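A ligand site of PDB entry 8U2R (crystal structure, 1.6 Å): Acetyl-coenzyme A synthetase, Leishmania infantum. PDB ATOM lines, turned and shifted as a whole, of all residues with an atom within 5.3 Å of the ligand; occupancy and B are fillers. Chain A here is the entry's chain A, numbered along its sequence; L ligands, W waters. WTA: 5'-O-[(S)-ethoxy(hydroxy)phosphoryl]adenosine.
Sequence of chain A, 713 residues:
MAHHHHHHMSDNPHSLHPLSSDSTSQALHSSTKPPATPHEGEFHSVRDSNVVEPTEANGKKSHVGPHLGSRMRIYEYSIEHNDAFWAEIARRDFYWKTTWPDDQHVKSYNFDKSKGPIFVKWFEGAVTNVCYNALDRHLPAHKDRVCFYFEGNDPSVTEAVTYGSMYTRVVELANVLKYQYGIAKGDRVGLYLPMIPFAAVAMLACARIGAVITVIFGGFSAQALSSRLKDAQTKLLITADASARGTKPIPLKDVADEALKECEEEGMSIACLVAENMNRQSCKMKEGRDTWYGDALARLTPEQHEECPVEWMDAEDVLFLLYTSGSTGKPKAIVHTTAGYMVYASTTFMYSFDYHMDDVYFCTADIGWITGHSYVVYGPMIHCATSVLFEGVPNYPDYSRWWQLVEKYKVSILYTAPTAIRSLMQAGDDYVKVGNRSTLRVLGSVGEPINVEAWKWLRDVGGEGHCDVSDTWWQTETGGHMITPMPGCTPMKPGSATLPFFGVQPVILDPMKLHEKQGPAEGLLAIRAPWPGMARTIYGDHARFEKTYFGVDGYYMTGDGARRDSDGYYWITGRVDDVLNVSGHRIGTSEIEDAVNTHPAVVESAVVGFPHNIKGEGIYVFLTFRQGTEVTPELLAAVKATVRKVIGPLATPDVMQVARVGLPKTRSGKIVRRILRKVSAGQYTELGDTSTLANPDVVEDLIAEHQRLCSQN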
ATOM      1  N   THR A 324     -23.511 -29.408  -9.328  1.00  0.00           N
ATOM      2  CA  THR A 324     -22.328 -29.513 -10.168  1.00  0.00           C
ATOM      3  C   THR A 324     -22.544 -30.625 -11.184  1.00  0.00           C
ATOM      4  O   THR A 324     -22.946 -31.737 -10.827  1.00  0.00           O
ATOM      5  CB  THR A 324     -21.104 -29.793  -9.290  1.00  0.00           C
ATOM      6  OG1 THR A 324     -20.985 -28.756  -8.300  1.00  0.00           O
ATOM      7  CG2 THR A 324     -19.824 -29.798 -10.118  1.00  0.00           C
ATOM      8  N   ILE A 370     -18.046 -22.437  -8.037  1.00  0.00           N
ATOM      9  CA  ILE A 370     -17.202 -22.567  -6.858  1.00  0.00           C
ATOM     10  C   ILE A 370     -16.163 -21.447  -6.787  1.00  0.00           C
ATOM     11  O   ILE A 370     -15.793 -21.018  -5.693  1.00  0.00           O
ATOM     12  CB  ILE A 370     -16.535 -23.961  -6.850  1.00  0.00           C
ATOM     13  CG1 ILE A 370     -15.826 -24.231  -5.522  1.00  0.00           C
ATOM     14  CG2 ILE A 370     -15.581 -24.104  -8.055  1.00  0.00           C
ATOM     15  CD1 ILE A 370     -16.752 -24.458  -4.313  1.00  0.00           C
ATOM     16  N   THR A 371     -15.675 -20.952  -7.915  1.00  0.00           N
ATOM     17  CA  THR A 371     -14.655 -19.917  -7.876  1.00  0.00           C
ATOM     18  C   THR A 371     -15.164 -18.669  -7.166  1.00  0.00           C
ATOM     19  O   THR A 371     -14.429 -18.008  -6.414  1.00  0.00           O
ATOM     20  CB  THR A 371     -14.187 -19.590  -9.296  1.00  0.00           C
ATOM     21  OG1 THR A 371     -13.701 -20.794  -9.909  1.00  0.00           O
ATOM     22  CG2 THR A 371     -13.059 -18.580  -9.292  1.00  0.00           C
ATOM     23  N   SER A 445      -5.412 -17.450 -13.475  1.00  0.00           N
ATOM     24  CA  SER A 445      -6.267 -18.092 -14.477  1.00  0.00           C
ATOM     25  C   SER A 445      -6.877 -19.349 -13.874  1.00  0.00           C
ATOM     26  O   SER A 445      -6.184 -20.132 -13.228  1.00  0.00           O
ATOM     27  CB  SER A 445      -5.434 -18.432 -15.716  1.00  0.00           C
ATOM     28  OG  SER A 445      -6.219 -18.995 -16.744  1.00  0.00           O
ATOM     29  N   VAL A 446      -8.165 -19.574 -14.118  1.00  0.00           N
ATOM     30  CA  VAL A 446      -8.870 -20.724 -13.566  1.00  0.00           C
ATOM     31  C   VAL A 446      -9.879 -21.266 -14.564  1.00  0.00           C
ATOM     32  O   VAL A 446     -10.494 -20.530 -15.330  1.00  0.00           O
ATOM     33  CB  VAL A 446      -9.601 -20.371 -12.259  1.00  0.00           C
ATOM     34  CG1 VAL A 446     -10.541 -19.166 -12.443  1.00  0.00           C
ATOM     35  CG2 VAL A 446     -10.411 -21.581 -11.748  1.00  0.00           C
ATOM     36  N   GLY A 447     -10.030 -22.586 -14.529  1.00  0.00           N
ATOM     37  CA  GLY A 447     -11.227 -23.238 -15.013  1.00  0.00           C
ATOM     38  C   GLY A 447     -11.047 -24.047 -16.276  1.00  0.00           C
ATOM     39  O   GLY A 447     -11.920 -24.874 -16.581  1.00  0.00           O
ATOM     40  N   GLU A 448      -9.968 -23.829 -17.010  1.00  0.00           N
ATOM     41  CA  GLU A 448      -9.747 -24.475 -18.293  1.00  0.00           C
ATOM     42  C   GLU A 448      -8.260 -24.365 -18.629  1.00  0.00           C
ATOM     43  O   GLU A 448      -7.565 -23.513 -18.072  1.00  0.00           O
ATOM     44  CB  GLU A 448     -10.605 -23.837 -19.398  1.00  0.00           C
ATOM     45  CG  GLU A 448     -10.735 -22.351 -19.223  1.00  0.00           C
ATOM     46  CD  GLU A 448     -11.751 -21.654 -20.115  1.00  0.00           C
ATOM     47  OE1 GLU A 448     -11.784 -21.992 -21.327  1.00  0.00           O
ATOM     48  OE2 GLU A 448     -12.403 -20.707 -19.569  1.00  0.00           O
ATOM     49  N   PRO A 449      -7.765 -25.209 -19.526  1.00  0.00           N
ATOM     50  CA  PRO A 449      -6.370 -25.070 -19.970  1.00  0.00           C
ATOM     51  C   PRO A 449      -6.160 -23.711 -20.629  1.00  0.00           C
ATOM     52  O   PRO A 449      -7.080 -23.109 -21.159  1.00  0.00           O
ATOM     53  CB  PRO A 449      -6.191 -26.236 -20.953  1.00  0.00           C
ATOM     54  CG  PRO A 449      -7.289 -27.240 -20.545  1.00  0.00           C
ATOM     55  CD  PRO A 449      -8.432 -26.361 -20.155  1.00  0.00           C
ATOM     56  N   ASP A 471      -1.748 -20.012 -12.676  1.00  0.00           N
ATOM     57  CA  ASP A 471      -2.705 -20.892 -13.355  1.00  0.00           C
ATOM     58  C   ASP A 471      -3.079 -21.956 -12.339  1.00  0.00           C
ATOM     59  O   ASP A 471      -2.282 -22.859 -12.044  1.00  0.00           O
ATOM     60  CB  ASP A 471      -2.090 -21.468 -14.624  1.00  0.00           C
ATOM     61  CG  ASP A 471      -2.991 -22.478 -15.307  1.00  0.00           C
ATOM     62  OD1 ASP A 471      -4.173 -22.603 -14.907  1.00  0.00           O
ATOM     63  OD2 ASP A 471      -2.483 -23.149 -16.255  1.00  0.00           O
ATOM     64  N   THR A 472      -4.291 -21.822 -11.771  1.00  0.00           N
ATOM     65  CA  THR A 472      -4.735 -22.628 -10.642  1.00  0.00           C
ATOM     66  C   THR A 472      -5.634 -23.760 -11.101  1.00  0.00           C
ATOM     67  O   THR A 472      -6.742 -23.513 -11.561  1.00  0.00           O
ATOM     68  CB  THR A 472      -5.502 -21.793  -9.615  1.00  0.00           C
ATOM     69  OG1 THR A 472      -6.692 -21.249 -10.198  1.00  0.00           O
ATOM     70  CG2 THR A 472      -4.670 -20.664  -9.087  1.00  0.00           C
ATOM     71  N   TRP A 473      -5.175 -25.011 -10.941  1.00  0.00           N
ATOM     72  CA  TRP A 473      -6.032 -26.172 -11.195  1.00  0.00           C
ATOM     73  C   TRP A 473      -6.683 -26.625  -9.893  1.00  0.00           C
ATOM     74  O   TRP A 473      -6.012 -26.741  -8.850  1.00  0.00           O
ATOM     75  CB  TRP A 473      -5.287 -27.359 -11.850  1.00  0.00           C
ATOM     76  CG  TRP A 473      -6.231 -28.524 -11.965  1.00  0.00           C
ATOM     77  CD1 TRP A 473      -7.115 -28.787 -12.950  1.00  0.00           C
ATOM     78  CD2 TRP A 473      -6.451 -29.540 -10.947  1.00  0.00           C
ATOM     79  NE1 TRP A 473      -7.871 -29.894 -12.643  1.00  0.00           N
ATOM     80  CE2 TRP A 473      -7.476 -30.381 -11.420  1.00  0.00           C
ATOM     81  CE3 TRP A 473      -5.894 -29.809  -9.696  1.00  0.00           C
ATOM     82  CZ2 TRP A 473      -7.961 -31.459 -10.689  1.00  0.00           C
ATOM     83  CZ3 TRP A 473      -6.353 -30.898  -8.983  1.00  0.00           C
ATOM     84  CH2 TRP A 473      -7.384 -31.706  -9.483  1.00  0.00           C
ATOM     85  N   TRP A 474      -7.998 -26.860  -9.973  1.00  0.00           N
ATOM     86  CA  TRP A 474      -8.807 -27.378  -8.881  1.00  0.00           C
ATOM     87  C   TRP A 474     -10.229 -27.601  -9.409  1.00  0.00           C
ATOM     88  O   TRP A 474     -10.479 -27.467 -10.618  1.00  0.00           O
ATOM     89  CB  TRP A 474      -8.813 -26.410  -7.687  1.00  0.00           C
ATOM     90  CG  TRP A 474      -9.357 -25.043  -7.969  1.00  0.00           C
ATOM     91  CD1 TRP A 474      -8.853 -24.097  -8.821  1.00  0.00           C
ATOM     92  CD2 TRP A 474     -10.492 -24.444  -7.332  1.00  0.00           C
ATOM     93  NE1 TRP A 474      -9.631 -22.957  -8.788  1.00  0.00           N
ATOM     94  CE2 TRP A 474     -10.644 -23.151  -7.876  1.00  0.00           C
ATOM     95  CE3 TRP A 474     -11.410 -24.879  -6.371  1.00  0.00           C
ATOM     96  CZ2 TRP A 474     -11.679 -22.303  -7.481  1.00  0.00           C
ATOM     97  CZ3 TRP A 474     -12.427 -24.030  -5.984  1.00  0.00           C
ATOM     98  CH2 TRP A 474     -12.542 -22.756  -6.547  1.00  0.00           C
ATOM     99  N   GLN A 475     -11.160 -27.985  -8.530  1.00  0.00           N
ATOM    100  CA  GLN A 475     -12.504 -28.347  -8.933  1.00  0.00           C
ATOM    101  C   GLN A 475     -13.467 -28.022  -7.798  1.00  0.00           C
ATOM    102  O   GLN A 475     -13.062 -27.863  -6.648  1.00  0.00           O
ATOM    103  CB  GLN A 475     -12.646 -29.855  -9.205  1.00  0.00           C
ATOM    104  CG  GLN A 475     -11.442 -30.545  -9.701  1.00  0.00           C
ATOM    105  CD  GLN A 475     -11.658 -32.030  -9.804  1.00  0.00           C
ATOM    106  OE1 GLN A 475     -11.587 -32.770  -8.824  1.00  0.00           O
ATOM    107  NE2 GLN A 475     -11.887 -32.479 -11.001  1.00  0.00           N
ATOM    108  N   THR A 476     -14.760 -28.033  -8.120  1.00  0.00           N
ATOM    109  CA  THR A 476     -15.785 -27.847  -7.090  1.00  0.00           C
ATOM    110  C   THR A 476     -15.526 -28.788  -5.915  1.00  0.00           C
ATOM    111  O   THR A 476     -15.563 -28.373  -4.738  1.00  0.00           O
ATOM    112  CB  THR A 476     -17.179 -28.061  -7.672  1.00  0.00           C
ATOM    113  OG1 THR A 476     -17.393 -27.131  -8.739  1.00  0.00           O
ATOM    114  CG2 THR A 476     -18.208 -27.824  -6.594  1.00  0.00           C
ATOM    115  N   GLU A 477     -15.224 -30.048  -6.217  1.00  0.00           N
ATOM    116  CA  GLU A 477     -15.018 -31.070  -5.207  1.00  0.00           C
ATOM    117  C   GLU A 477     -13.787 -30.864  -4.350  1.00  0.00           C
ATOM    118  O   GLU A 477     -13.652 -31.529  -3.317  1.00  0.00           O
ATOM    119  CB  GLU A 477     -14.920 -32.427  -5.903  1.00  0.00           C
ATOM    120  CG  GLU A 477     -16.149 -32.824  -6.707  1.00  0.00           C
ATOM    121  CD  GLU A 477     -16.081 -32.460  -8.173  1.00  0.00           C
ATOM    122  OE1 GLU A 477     -15.454 -31.468  -8.555  1.00  0.00           O
ATOM    123  OE2 GLU A 477     -16.693 -33.200  -8.963  1.00  0.00           O
ATOM    124  N   THR A 558      -9.937 -37.485 -10.007  1.00  0.00           N
ATOM    125  CA  THR A 558     -10.401 -36.131 -10.354  1.00  0.00           C
ATOM    126  C   THR A 558     -11.374 -36.137 -11.524  1.00  0.00           C
ATOM    127  O   THR A 558     -12.216 -35.239 -11.600  1.00  0.00           O
ATOM    128  CB  THR A 558      -9.223 -35.204 -10.709  1.00  0.00           C
ATOM    129  OG1 THR A 558      -8.562 -35.664 -11.890  1.00  0.00           O
ATOM    130  CG2 THR A 558      -8.242 -35.142  -9.598  1.00  0.00           C
ATOM    131  N   ASP A 560      -9.948 -35.709 -14.467  1.00  0.00           N
ATOM    132  CA  ASP A 560      -9.050 -35.078 -15.427  1.00  0.00           C
ATOM    133  C   ASP A 560      -7.885 -36.008 -15.764  1.00  0.00           C
ATOM    134  O   ASP A 560      -7.514 -36.898 -14.999  1.00  0.00           O
ATOM    135  CB  ASP A 560      -8.461 -33.781 -14.879  1.00  0.00           C
ATOM    136  CG  ASP A 560      -9.440 -32.656 -14.868  1.00  0.00           C
ATOM    137  OD1 ASP A 560     -10.052 -32.391 -15.919  1.00  0.00           O
ATOM    138  OD2 ASP A 560      -9.566 -32.032 -13.800  1.00  0.00           O
ATOM    139  N   ILE A 572      -2.452 -30.017 -17.151  1.00  0.00           N
ATOM    140  CA  ILE A 572      -3.804 -30.584 -17.194  1.00  0.00           C
ATOM    141  C   ILE A 572      -4.278 -30.659 -18.640  1.00  0.00           C
ATOM    142  O   ILE A 572      -4.321 -29.638 -19.332  1.00  0.00           O
ATOM    143  CB  ILE A 572      -4.771 -29.715 -16.376  1.00  0.00           C
ATOM    144  CG1 ILE A 572      -4.206 -29.436 -15.021  1.00  0.00           C
ATOM    145  CG2 ILE A 572      -6.158 -30.420 -16.316  1.00  0.00           C
ATOM    146  CD1 ILE A 572      -4.114 -30.632 -14.134  1.00  0.00           C
ATOM    147  N   GLY A 574      -7.400 -32.008 -19.582  1.00  0.00           N
ATOM    148  CA  GLY A 574      -8.840 -31.932 -19.712  1.00  0.00           C
ATOM    149  C   GLY A 574      -9.551 -33.176 -19.192  1.00  0.00           C
ATOM    150  O   GLY A 574      -8.950 -34.175 -18.792  1.00  0.00           O
ATOM    151  N   ARG A 575     -10.887 -33.109 -19.230  1.00  0.00           N
ATOM    152  CA  ARG A 575     -11.674 -34.202 -18.695  1.00  0.00           C
ATOM    153  C   ARG A 575     -11.453 -35.468 -19.509  1.00  0.00           C
ATOM    154  O   ARG A 575     -11.310 -35.422 -20.739  1.00  0.00           O
ATOM    155  CB  ARG A 575     -13.169 -33.871 -18.705  1.00  0.00           C
ATOM    156  CG  ARG A 575     -13.574 -32.661 -17.888  1.00  0.00           C
ATOM    157  CD  ARG A 575     -13.388 -32.821 -16.415  1.00  0.00           C
ATOM    158  NE  ARG A 575     -14.234 -33.811 -15.775  1.00  0.00           N
ATOM    159  CZ  ARG A 575     -14.540 -33.814 -14.481  1.00  0.00           C
ATOM    160  NH1 ARG A 575     -14.124 -32.848 -13.675  1.00  0.00           N
ATOM    161  NH2 ARG A 575     -15.255 -34.809 -13.984  1.00  0.00           N
ATOM    162  N   ASN A 581     -16.602 -28.426 -20.961  1.00  0.00           N
ATOM    163  CA  ASN A 581     -16.077 -27.169 -20.435  1.00  0.00           C
ATOM    164  C   ASN A 581     -16.343 -26.091 -21.485  1.00  0.00           C
ATOM    165  O   ASN A 581     -15.532 -25.904 -22.398  1.00  0.00           O
ATOM    166  CB  ASN A 581     -14.598 -27.322 -20.135  1.00  0.00           C
ATOM    167  CG  ASN A 581     -14.036 -26.161 -19.402  1.00  0.00           C
ATOM    168  OD1 ASN A 581     -14.550 -25.048 -19.499  1.00  0.00           O
ATOM    169  ND2 ASN A 581     -12.944 -26.391 -18.662  1.00  0.00           N
ATOM    170  N   ARG A 586     -18.716 -25.738 -16.448  1.00  0.00           N
ATOM    171  CA  ARG A 586     -18.727 -27.196 -16.389  1.00  0.00           C
ATOM    172  C   ARG A 586     -20.166 -27.682 -16.608  1.00  0.00           C
ATOM    173  O   ARG A 586     -21.052 -27.339 -15.824  1.00  0.00           O
ATOM    174  CB  ARG A 586     -18.199 -27.608 -15.024  1.00  0.00           C
ATOM    175  CG  ARG A 586     -18.272 -29.059 -14.732  1.00  0.00           C
ATOM    176  CD  ARG A 586     -17.578 -29.340 -13.391  1.00  0.00           C
ATOM    177  NE  ARG A 586     -17.859 -30.698 -12.957  1.00  0.00           N
ATOM    178  CZ  ARG A 586     -17.295 -31.280 -11.907  1.00  0.00           C
ATOM    179  NH1 ARG A 586     -16.354 -30.677 -11.206  1.00  0.00           N
ATOM    180  NH2 ARG A 586     -17.686 -32.499 -11.572  1.00  0.00           N
HETATM  181  C1' WTA L   1     -11.068 -27.845 -15.339  1.00  0.00           C
HETATM  182  C1P WTA L   1     -13.635 -24.765 -11.345  1.00  0.00           C
HETATM  183  C2  WTA L   1      -7.109 -26.780 -16.759  1.00  0.00           C
HETATM  184  C2' WTA L   1     -10.760 -29.315 -15.078  1.00  0.00           C
HETATM  185  C2P WTA L   1     -12.537 -24.369 -10.445  1.00  0.00           C
HETATM  186  C3' WTA L   1     -11.506 -29.533 -13.760  1.00  0.00           C
HETATM  187  C4  WTA L   1      -8.835 -26.700 -15.399  1.00  0.00           C
HETATM  188  C4' WTA L   1     -12.762 -28.672 -13.945  1.00  0.00           C
HETATM  189  C5  WTA L   1      -8.224 -25.764 -14.592  1.00  0.00           C
HETATM  190  C5' WTA L   1     -13.386 -28.224 -12.652  1.00  0.00           C
HETATM  191  C6  WTA L   1      -6.945 -25.327 -14.960  1.00  0.00           C
HETATM  192  C8  WTA L   1     -10.108 -26.156 -13.702  1.00  0.00           C
HETATM  193  N1  WTA L   1      -6.401 -25.875 -16.077  1.00  0.00           N
HETATM  194  N3  WTA L   1      -8.334 -27.261 -16.514  1.00  0.00           N
HETATM  195  N6  WTA L   1      -6.283 -24.389 -14.275  1.00  0.00           N
HETATM  196  N7  WTA L   1      -9.042 -25.419 -13.522  1.00  0.00           N
HETATM  197  N9  WTA L   1     -10.046 -26.953 -14.819  1.00  0.00           N
HETATM  198  O1P WTA L   1     -16.321 -25.854 -12.224  1.00  0.00           O
HETATM  199  O2' WTA L   1     -11.301 -30.110 -16.116  1.00  0.00           O
HETATM  200  O2P WTA L   1     -15.774 -27.928 -10.801  1.00  0.00           O
HETATM  201  O3' WTA L   1     -11.845 -30.893 -13.483  1.00  0.00           O
HETATM  202  O3P WTA L   1     -14.220 -25.997 -10.840  1.00  0.00           O
HETATM  203  O4' WTA L   1     -12.296 -27.519 -14.697  1.00  0.00           O
HETATM  204  O5' WTA L   1     -14.558 -27.406 -12.926  1.00  0.00           O
HETATM  205  P   WTA L   1     -15.337 -26.816 -11.663  1.00  0.00           P
HETATM  206  O   HOH W   1     -19.117 -26.197 -11.911  1.00  0.00           O
HETATM  207  O   HOH W   2      -6.392 -21.649 -16.357  1.00  0.00           O
HETATM  208  O   HOH W   3     -14.566 -25.352 -15.234  1.00  0.00           O
HETATM  209  O   HOH W   4      -3.838 -25.207 -17.108  1.00  0.00           O
HETATM  210  O   HOH W   5     -13.074 -29.216 -18.006  1.00  0.00           O
HETATM  211  O   HOH W   6      -9.302 -29.161 -18.365  1.00  0.00           O
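OD2 of Asp 560 sits at hydrogen-bond distance from O3' of the ligand (2.6 Å). An oxygen (O2P) of the ligand sits at hydrogen-bond distance from the backbone NH (N) of Thr 476 (2.9 Å). O2P of the ligand lies within hydrogen-bond range of OG1 of Thr 476 (2.7 Å). The side-chain carboxylate (OD1) of Asp 471 sits at hydrogen-bond distance from a nitrogen (N6) of the ligand. An oxygen (O2P) of the ligand is in salt-bridge range of the guanidinium group (NH1) of Arg 586, at 2.8 Å. O of Thr 472 sits at hydrogen-bond distance from N6 of the ligand (2.9 Å). The side-chain amide nitrogen of Gln 475 is in hydrogen-bond range of an oxygen (O3') of the ligand (2.9 Å). An oxygen (O3') of the ligand is in hydrogen-bond range of the guanidinium group (NH1) of Arg 575, at 3.0 Å. The backbone NH (N) of Gly 447 sits at hydrogen-bond distance from a nitrogen (N7) of the ligand (3.2 Å).
N of Arg 575 sits close to OD1 of Asp 560 (3.5 Å). The side-chain carboxylate (OD2) of Asp 560 is in hydrogen-bond range of the indole nitrogen (NE1) of Trp 473 (3.0 Å). The side-chain hydroxyl (OG1) of Thr 558 sits at hydrogen-bond distance from the backbone NH (N) of Asp 560, at 2.9 Å. The guanidinium group of Arg 586 lies within salt-bridge range of the side-chain carboxylate of Glu 477 (2.9 Å). The backbone NH (N) of Thr 472 lies within hydrogen-bond range of the backbone carbonyl oxygen (O) of Ser 445 (2.9 Å). O of Thr 558 lies within hydrogen-bond range of NE2 of Gln 475 (2.8 Å). ND2 of Asn 581 is in hydrogen-bond range of O of Gly 447, at 2.8 Å.
N1 of the ligand sits close to O of Glu 448 (3.3 Å). Ile 370 touches the ligand (CG2 to O3P, 3.6 Å). Thr 371 touches the ligand (OG1 to C2P, 3.8 Å). Val 446 touches the ligand. N of Pro 449 touches C2 of the ligand, 3.2 Å away. Trp 473 touches the ligand (CA to N6, 3.6 Å). Trp 474 touches the ligand. Ile 572 touches the ligand (CB to C2, 3.8 Å). Hydrophobic or aromatic side chains within 4 Å of the ligand: Ile 370, Val 446, Pro 449, Trp 473, Trp 474 and Ile 572. Within 4 Å of the ligand: Ile 370, Thr 371, Val 446, Gly 447, Glu 448, Pro 449, Asp 471, Thr 472, Trp 473, Trp 474, Gln 475, Thr 476, Asp 560, Ile 572, Arg 575 and Arg 586.
Water W5 bridges O2' of the ligand (2.7 Å) and ND2 of Asn 581 (2.9 Å). Water W4 bridges the side-chain carboxylate (OD2) of Asp 471 and a nitrogen (N1) of the ligand. Water W3 bridges the backbone carbonyl oxygen of Gly 447 (3.0 Å) and an oxygen (O5') of the ligand (3.1 Å). Water W2 lies within hydrogen-bond range of OG of Ser 445, O of Glu 448, OD1 of Asp 471 and N6 of the ligand.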
